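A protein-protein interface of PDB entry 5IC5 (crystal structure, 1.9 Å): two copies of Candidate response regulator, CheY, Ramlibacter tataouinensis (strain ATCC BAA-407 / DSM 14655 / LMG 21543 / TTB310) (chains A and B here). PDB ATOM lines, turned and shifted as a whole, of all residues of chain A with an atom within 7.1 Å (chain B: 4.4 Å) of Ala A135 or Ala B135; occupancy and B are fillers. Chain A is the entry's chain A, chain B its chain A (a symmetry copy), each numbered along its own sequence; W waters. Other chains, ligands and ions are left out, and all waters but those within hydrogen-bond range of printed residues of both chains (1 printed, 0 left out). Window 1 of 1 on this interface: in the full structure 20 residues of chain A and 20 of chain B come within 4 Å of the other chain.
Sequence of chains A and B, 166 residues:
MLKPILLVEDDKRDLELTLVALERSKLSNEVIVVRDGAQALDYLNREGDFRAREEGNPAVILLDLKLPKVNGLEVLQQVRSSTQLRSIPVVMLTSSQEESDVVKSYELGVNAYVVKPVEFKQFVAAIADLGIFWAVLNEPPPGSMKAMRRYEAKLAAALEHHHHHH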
ATOM      1  N   MET A   1      17.623 -32.600 -22.756  1.00  0.00           N
ATOM      2  CA  MET A   1      17.855 -31.256 -23.262  1.00  0.00           C
ATOM      3  C   MET A   1      18.234 -31.250 -24.747  1.00  0.00           C
ATOM      4  O   MET A   1      17.675 -30.500 -25.529  1.00  0.00           O
ATOM      5  CB  MET A   1      18.953 -30.585 -22.456  1.00  0.00           C
ATOM      6  CG  MET A   1      19.293 -29.208 -22.948  1.00  0.00           C
ATOM      7  SD  MET A   1      20.428 -28.388 -21.815  1.00  0.00           S
ATOM      8  CE  MET A   1      20.897 -27.012 -22.850  1.00  0.00           C
ATOM      9  N   LEU A   2      19.197 -32.086 -25.119  1.00  0.00           N
ATOM     10  CA  LEU A   2      19.622 -32.209 -26.503  1.00  0.00           C
ATOM     11  C   LEU A   2      18.630 -33.092 -27.235  1.00  0.00           C
ATOM     12  O   LEU A   2      18.367 -34.206 -26.806  1.00  0.00           O
ATOM     13  CB  LEU A   2      21.027 -32.813 -26.600  1.00  0.00           C
ATOM     14  CG  LEU A   2      22.025 -32.047 -25.717  1.00  0.00           C
ATOM     15  CD1 LEU A   2      23.389 -32.682 -25.761  1.00  0.00           C
ATOM     16  CD2 LEU A   2      22.062 -30.615 -26.246  1.00  0.00           C
ATOM     17  N   LYS A   3      18.107 -32.603 -28.349  1.00  0.00           N
ATOM     18  CA  LYS A   3      17.135 -33.399 -29.116  1.00  0.00           C
ATOM     19  C   LYS A   3      17.825 -34.326 -30.120  1.00  0.00           C
ATOM     20  O   LYS A   3      18.942 -34.061 -30.552  1.00  0.00           O
ATOM     21  CB  LYS A   3      16.188 -32.448 -29.824  1.00  0.00           C
ATOM     22  CG  LYS A   3      15.615 -31.459 -28.797  1.00  0.00           C
ATOM     23  CD  LYS A   3      14.499 -30.660 -29.369  1.00  0.00           C
ATOM     24  CE  LYS A   3      14.929 -29.912 -30.591  1.00  0.00           C
ATOM     25  NZ  LYS A   3      13.822 -28.981 -30.970  1.00  0.00           N
ATOM     26  N   ILE A   5      18.853 -36.509 -33.615  1.00  0.00           N
ATOM     27  CA  ILE A   5      18.937 -36.276 -35.046  1.00  0.00           C
ATOM     28  C   ILE A   5      18.288 -37.484 -35.736  1.00  0.00           C
ATOM     29  O   ILE A   5      18.593 -38.632 -35.404  1.00  0.00           O
ATOM     30  CB  ILE A   5      20.391 -36.131 -35.515  1.00  0.00           C
ATOM     31  CG1 ILE A   5      21.020 -34.862 -34.917  1.00  0.00           C
ATOM     32  CG2 ILE A   5      20.472 -36.043 -37.031  1.00  0.00           C
ATOM     33  CD1 ILE A   5      22.577 -34.885 -35.087  1.00  0.00           C
ATOM     34  N   LYS A  26      32.098 -36.183 -34.137  1.00  0.00           N
ATOM     35  CA  LYS A  26      31.824 -36.061 -32.701  1.00  0.00           C
ATOM     36  C   LYS A  26      30.544 -35.240 -32.393  1.00  0.00           C
ATOM     37  O   LYS A  26      30.366 -34.767 -31.275  1.00  0.00           O
ATOM     38  CB  LYS A  26      33.044 -35.471 -31.972  1.00  0.00           C
ATOM     39  CG  LYS A  26      34.267 -36.453 -31.999  1.00  0.00           C
ATOM     40  CD  LYS A  26      35.299 -36.119 -30.914  1.00  0.00           C
ATOM     41  CE  LYS A  26      36.497 -36.995 -31.065  1.00  0.00           C
ATOM     42  NZ  LYS A  26      37.202 -36.507 -32.273  1.00  0.00           N
ATOM     43  N   LEU A  27      29.659 -35.107 -33.377  1.00  0.00           N
ATOM     44  CA  LEU A  27      28.346 -34.477 -33.172  1.00  0.00           C
ATOM     45  C   LEU A  27      27.572 -35.397 -32.264  1.00  0.00           C
ATOM     46  O   LEU A  27      27.463 -36.594 -32.586  1.00  0.00           O
ATOM     47  CB  LEU A  27      27.629 -34.267 -34.521  1.00  0.00           C
ATOM     48  CG  LEU A  27      26.186 -33.729 -34.522  1.00  0.00           C
ATOM     49  CD1 LEU A  27      26.112 -32.425 -33.720  1.00  0.00           C
ATOM     50  CD2 LEU A  27      25.745 -33.490 -35.959  1.00  0.00           C
ATOM     51  N   SER A  28      27.057 -34.897 -31.134  1.00  0.00           N
ATOM     52  CA  SER A  28      26.658 -35.833 -30.064  1.00  0.00           C
ATOM     53  C   SER A  28      25.167 -35.974 -29.762  1.00  0.00           C
ATOM     54  O   SER A  28      24.816 -36.689 -28.824  1.00  0.00           O
ATOM     55  CB  SER A  28      27.344 -35.443 -28.754  1.00  0.00           C
ATOM     56  OG  SER A  28      28.733 -35.653 -28.857  1.00  0.00           O
ATOM     57  N   ASN A  29      24.306 -35.244 -30.471  1.00  0.00           N
ATOM     58  CA  ASN A  29      22.866 -35.514 -30.350  1.00  0.00           C
ATOM     59  C   ASN A  29      22.625 -36.991 -30.670  1.00  0.00           C
ATOM     60  O   ASN A  29      23.286 -37.574 -31.550  1.00  0.00           O
ATOM     61  CB  ASN A  29      22.045 -34.675 -31.311  1.00  0.00           C
ATOM     62  CG  ASN A  29      22.334 -33.229 -31.232  1.00  0.00           C
ATOM     63  OD1 ASN A  29      23.441 -32.766 -31.595  1.00  0.00           O
ATOM     64  ND2 ASN A  29      21.304 -32.452 -30.877  1.00  0.00           N
ATOM     65  N   PHE A 133      22.018 -23.156 -33.704  1.00  0.00           N
ATOM     66  CA  PHE A 133      22.800 -22.964 -32.489  1.00  0.00           C
ATOM     67  C   PHE A 133      23.500 -24.273 -32.159  1.00  0.00           C
ATOM     68  O   PHE A 133      23.056 -25.351 -32.562  1.00  0.00           O
ATOM     69  CB  PHE A 133      21.924 -22.473 -31.337  1.00  0.00           C
ATOM     70  CG  PHE A 133      21.359 -21.109 -31.589  1.00  0.00           C
ATOM     71  CD1 PHE A 133      22.084 -19.979 -31.256  1.00  0.00           C
ATOM     72  CD2 PHE A 133      20.145 -20.955 -32.241  1.00  0.00           C
ATOM     73  CE1 PHE A 133      21.583 -18.694 -31.522  1.00  0.00           C
ATOM     74  CE2 PHE A 133      19.643 -19.699 -32.519  1.00  0.00           C
ATOM     75  CZ  PHE A 133      20.369 -18.571 -32.182  1.00  0.00           C
ATOM     76  N   TRP A 134      24.611 -24.181 -31.432  1.00  0.00           N
ATOM     77  CA  TRP A 134      25.326 -25.402 -31.082  1.00  0.00           C
ATOM     78  C   TRP A 134      26.134 -25.160 -29.802  1.00  0.00           C
ATOM     79  O   TRP A 134      26.276 -24.006 -29.349  1.00  0.00           O
ATOM     80  CB  TRP A 134      26.220 -25.854 -32.254  1.00  0.00           C
ATOM     81  CG  TRP A 134      27.281 -24.822 -32.644  1.00  0.00           C
ATOM     82  CD1 TRP A 134      27.074 -23.578 -33.216  1.00  0.00           C
ATOM     83  CD2 TRP A 134      28.711 -24.969 -32.526  1.00  0.00           C
ATOM     84  NE1 TRP A 134      28.275 -22.968 -33.445  1.00  0.00           N
ATOM     85  CE2 TRP A 134      29.294 -23.789 -33.029  1.00  0.00           C
ATOM     86  CE3 TRP A 134      29.553 -25.983 -32.026  1.00  0.00           C
ATOM     87  CZ2 TRP A 134      30.684 -23.585 -33.057  1.00  0.00           C
ATOM     88  CZ3 TRP A 134      30.938 -25.784 -32.076  1.00  0.00           C
ATOM     89  CH2 TRP A 134      31.485 -24.596 -32.584  1.00  0.00           C
ATOM     90  N   ALA A 135      26.667 -26.223 -29.217  1.00  0.00           N
ATOM     91  CA  ALA A 135      27.406 -26.056 -27.954  1.00  0.00           C
ATOM     92  C   ALA A 135      28.517 -27.111 -27.908  1.00  0.00           C
ATOM     93  O   ALA A 135      28.385 -28.152 -28.549  1.00  0.00           O
ATOM     94  CB  ALA A 135      26.455 -26.195 -26.773  1.00  0.00           C
ATOM     95  N   VAL A 136      29.618 -26.808 -27.231  1.00  0.00           N
ATOM     96  CA  VAL A 136      30.622 -27.831 -27.039  1.00  0.00           C
ATOM     97  C   VAL A 136      30.398 -28.599 -25.733  1.00  0.00           C
ATOM     98  O   VAL A 136      29.908 -28.034 -24.752  1.00  0.00           O
ATOM     99  CB  VAL A 136      32.047 -27.238 -27.070  1.00  0.00           C
ATOM    100  CG1 VAL A 136      32.372 -26.791 -28.517  1.00  0.00           C
ATOM    101  CG2 VAL A 136      32.156 -26.096 -26.179  1.00  0.00           C
ATOM    102  N   LEU A 137      30.834 -29.867 -25.754  1.00  0.00           N
ATOM    103  CA  LEU A 137      30.798 -30.792 -24.619  1.00  0.00           C
ATOM    104  C   LEU A 137      32.188 -31.446 -24.387  1.00  0.00           C
ATOM    105  O   LEU A 137      32.881 -31.864 -25.340  1.00  0.00           O
ATOM    106  CB  LEU A 137      29.747 -31.918 -24.861  1.00  0.00           C
ATOM    107  CG  LEU A 137      28.384 -31.652 -25.526  1.00  0.00           C
ATOM    108  CD1 LEU A 137      27.764 -33.005 -25.875  1.00  0.00           C
ATOM    109  CD2 LEU A 137      27.444 -30.909 -24.601  1.00  0.00           C
ATOM    110  N   PRO A 141      26.998 -37.245 -24.290  1.00  0.00           N
ATOM    111  CA  PRO A 141      25.983 -37.859 -23.428  1.00  0.00           C
ATOM    112  C   PRO A 141      26.010 -39.396 -23.593  1.00  0.00           C
ATOM    113  O   PRO A 141      26.104 -39.896 -24.720  1.00  0.00           O
ATOM    114  CB  PRO A 141      24.678 -37.248 -23.933  1.00  0.00           C
ATOM    115  CG  PRO A 141      25.110 -35.993 -24.705  1.00  0.00           C
ATOM    116  CD  PRO A 141      26.425 -36.331 -25.293  1.00  0.00           C
ATOM    117  N   LEU B   2      25.418 -27.815 -20.062  1.00  0.00           N
ATOM    118  CA  LEU B   2      26.440 -27.189 -20.883  1.00  0.00           C
ATOM    119  C   LEU B   2      27.325 -26.344 -19.988  1.00  0.00           C
ATOM    120  O   LEU B   2      26.831 -25.493 -19.263  1.00  0.00           O
ATOM    121  CB  LEU B   2      25.815 -26.314 -21.975  1.00  0.00           C
ATOM    122  CG  LEU B   2      24.770 -27.097 -22.786  1.00  0.00           C
ATOM    123  CD1 LEU B   2      24.109 -26.218 -23.814  1.00  0.00           C
ATOM    124  CD2 LEU B   2      25.512 -28.258 -23.444  1.00  0.00           C
ATOM    125  N   LEU B  27      27.736 -20.354 -31.275  1.00  0.00           N
ATOM    126  CA  LEU B  27      28.232 -21.268 -30.235  1.00  0.00           C
ATOM    127  C   LEU B  27      27.567 -20.848 -28.950  1.00  0.00           C
ATOM    128  O   LEU B  27      27.656 -19.658 -28.597  1.00  0.00           O
ATOM    129  CB  LEU B  27      29.769 -21.193 -30.135  1.00  0.00           C
ATOM    130  CG  LEU B  27      30.483 -21.984 -29.023  1.00  0.00           C
ATOM    131  CD1 LEU B  27      30.067 -23.459 -29.079  1.00  0.00           C
ATOM    132  CD2 LEU B  27      31.988 -21.853 -29.208  1.00  0.00           C
ATOM    133  N   SER B  28      26.883 -21.764 -28.253  1.00  0.00           N
ATOM    134  CA  SER B  28      25.914 -21.304 -27.239  1.00  0.00           C
ATOM    135  C   SER B  28      26.242 -21.567 -25.771  1.00  0.00           C
ATOM    136  O   SER B  28      25.414 -21.261 -24.913  1.00  0.00           O
ATOM    137  CB  SER B  28      24.545 -21.931 -27.510  1.00  0.00           C
ATOM    138  OG  SER B  28      24.012 -21.424 -28.711  1.00  0.00           O
ATOM    139  N   ASN B  29      27.378 -22.201 -25.480  1.00  0.00           N
ATOM    140  CA  ASN B  29      27.819 -22.278 -24.080  1.00  0.00           C
ATOM    141  C   ASN B  29      27.905 -20.855 -23.524  1.00  0.00           C
ATOM    142  O   ASN B  29      28.290 -19.908 -24.237  1.00  0.00           O
ATOM    143  CB  ASN B  29      29.184 -22.929 -23.946  1.00  0.00           C
ATOM    144  CG  ASN B  29      29.285 -24.238 -24.619  1.00  0.00           C
ATOM    145  OD1 ASN B  29      29.235 -24.334 -25.868  1.00  0.00           O
ATOM    146  ND2 ASN B  29      29.558 -25.278 -23.822  1.00  0.00           N
ATOM    147  N   TRP B 134      30.334 -32.131 -29.488  1.00  0.00           N
ATOM    148  CA  TRP B 134      29.478 -30.959 -29.623  1.00  0.00           C
ATOM    149  C   TRP B 134      28.055 -31.415 -29.967  1.00  0.00           C
ATOM    150  O   TRP B 134      27.829 -32.598 -30.289  1.00  0.00           O
ATOM    151  CB  TRP B 134      30.051 -29.998 -30.684  1.00  0.00           C
ATOM    152  CG  TRP B 134      30.160 -30.623 -32.078  1.00  0.00           C
ATOM    153  CD1 TRP B 134      31.004 -31.646 -32.476  1.00  0.00           C
ATOM    154  CD2 TRP B 134      29.427 -30.234 -33.257  1.00  0.00           C
ATOM    155  NE1 TRP B 134      30.827 -31.900 -33.807  1.00  0.00           N
ATOM    156  CE2 TRP B 134      29.866 -31.059 -34.311  1.00  0.00           C
ATOM    157  CE3 TRP B 134      28.427 -29.275 -33.516  1.00  0.00           C
ATOM    158  CZ2 TRP B 134      29.350 -30.959 -35.615  1.00  0.00           C
ATOM    159  CZ3 TRP B 134      27.931 -29.165 -34.820  1.00  0.00           C
ATOM    160  CH2 TRP B 134      28.392 -30.003 -35.848  1.00  0.00           C
ATOM    161  N   ALA B 135      27.101 -30.498 -29.907  1.00  0.00           N
ATOM    162  CA  ALA B 135      25.706 -30.893 -30.173  1.00  0.00           C
ATOM    163  C   ALA B 135      24.988 -29.702 -30.816  1.00  0.00           C
ATOM    164  O   ALA B 135      25.400 -28.563 -30.602  1.00  0.00           O
ATOM    165  CB  ALA B 135      25.031 -31.319 -28.876  1.00  0.00           C
ATOM    166  N   VAL B 136      23.987 -29.969 -31.648  1.00  0.00           N
ATOM    167  CA  VAL B 136      23.191 -28.875 -32.155  1.00  0.00           C
ATOM    168  C   VAL B 136      21.973 -28.607 -31.265  1.00  0.00           C
ATOM    169  O   VAL B 136      21.424 -29.533 -30.663  1.00  0.00           O
ATOM    170  CB  VAL B 136      22.742 -29.129 -33.610  1.00  0.00           C
ATOM    171  CG1 VAL B 136      23.976 -29.033 -34.540  1.00  0.00           C
ATOM    172  CG2 VAL B 136      22.137 -30.442 -33.747  1.00  0.00           C
ATOM    173  N   LEU B 137      21.553 -27.333 -31.269  1.00  0.00           N
ATOM    174  CA  LEU B 137      20.377 -26.830 -30.556  1.00  0.00           C
ATOM    175  C   LEU B 137      19.457 -26.013 -31.505  1.00  0.00           C
ATOM    176  O   LEU B 137      19.926 -25.191 -32.322  1.00  0.00           O
ATOM    177  CB  LEU B 137      20.804 -25.920 -29.364  1.00  0.00           C
ATOM    178  CG  LEU B 137      22.017 -26.239 -28.471  1.00  0.00           C
ATOM    179  CD1 LEU B 137      22.313 -24.999 -27.627  1.00  0.00           C
ATOM    180  CD2 LEU B 137      21.742 -27.404 -27.545  1.00  0.00           C
HETATM  181  O   HOH W   1      18.974 -30.129 -29.542  1.00  0.00           O
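The backbone carbonyl oxygen of Lys A26 lies within hydrogen-bond range of the backbone NH of Trp B134, 3.2 Å away.
N of Ser A28 sits at hydrogen-bond distance from O of Trp B134, at 2.6 Å.
N of Val B136 sits at hydrogen-bond distance from OD1 of Asn A29 (2.9 Å).
The backbone carbonyl oxygen (O) of Phe A133 lies within hydrogen-bond range of the backbone NH (N) of Leu B137, at 2.8 Å.
The backbone carbonyl oxygen of Trp A134 is in hydrogen-bond range of the backbone NH of Ser B28.
O of Ala B135 lies within hydrogen-bond range of N of Ala A135 (3.0 Å).
N of Val A136 sits at hydrogen-bond distance from OD1 of Asn B29 (2.9 Å).
The backbone NH of Leu A27 lies close to the indole nitrogen of Trp B134, 3.4 Å away.
NE1 of Trp A134 sits close to N of Leu B27, 3.4 Å away.
Of chain B, only Leu B2, Leu B27, Asn B29, Trp B134 and Ala B135 come within 4 Å of Ala A135.
Of chain A, only Leu A2 (3.8 Å), Leu A27 (3.9 Å), Asn A29 (3.3 Å), Trp A134 (3.2 Å) and Ala A135 (3.0 Å) come within 4 Å of Ala B135.
Printed residues of chain B within 4 Å of Leu A137: Leu B2.
Of the printed residues of chain A, Asn B29 touches Ala A135 (3.3 Å) and Val A136 (2.9 Å).
Printed residues of chain B within 4 Å of Asn A29: Ala B135 and Val B136.
The nearest printed residue of chain A that does not touch Val B136 is Trp A134 (4.2 Å).
Of the 14 printed residues of chain A, 11 touch a printed residue of chain B.
Printed residues of chain A that touch a printed residue of chain B: Met A1, Leu A2, Lys A26, Leu A27, Ser A28, Asn A29, Phe A133, Trp A134, Ala A135, Val A136 and Leu A137.
Hydrophobic or aromatic side chains of chain A that line the printed part of chain B: Met A1, Leu A2, Leu A27, Phe A133, Trp A134, Ala A135, Val A136 and Leu A137.
Of the 8 printed residues of chain B, 8 touch a printed residue of chain A.
Among the printed residues, 25 pairs touch across the chains.
Water W1 bridges the backbone carbonyl oxygen of Val B136 (2.8 Å) and the backbone NH of Lys A3 (2.9 Å).
ND2 of Asn A29 sits at hydrogen-bond distance from O of Lys A3, at 2.9 Å.
The backbone carbonyl oxygen (O) of Lys A26 lies within hydrogen-bond range of the side-chain hydroxyl (OG) of Ser A28, 3.0 Å away.
Among the printed residues, pairs that only touch across the chains: Ala A135 with Trp B134 (3.2 Å), Trp A134 with Ala B135 (3.2 Å), Asn A29 with Ala B135 (3.3 Å), Ala A135 with Asn B29 (3.3 Å), Met A1 with Leu B2 (3.4 Å), Leu A137 with Leu B2 (3.5 Å), Leu A2 with Leu B137 (3.5 Å), Phe A133 with Ser B28 (3.5 Å), Phe A133 with Val B136 (3.5 Å), Leu A2 with Ala B135 (3.8 Å), Ala A135 with Leu B2 (3.8 Å), Trp A134 with Trp B134 (3.8 Å), Val A136 with Leu B27 (3.9 Å), Leu A27 with Val B136 (3.9 Å), Ala A135 with Leu B27 (3.9 Å) and Leu A27 with Ala B135 (3.9 Å).
Leu A27 touches Trp B134, and with the chains exchanged Trp A134 touches Leu B27.
Ser A28 touches Trp B134, and with the chains exchanged Trp A134 touches Ser B28.
Asn A29 touches Ala B135, and with the chains exchanged Ala A135 touches Asn B29.
Asn A29 touches Val B136, and with the chains exchanged Val A136 touches Asn B29.
Of the 25 pairs that touch across the chains among the printed residues, 20 have their exchanged pair printed and touching as well.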
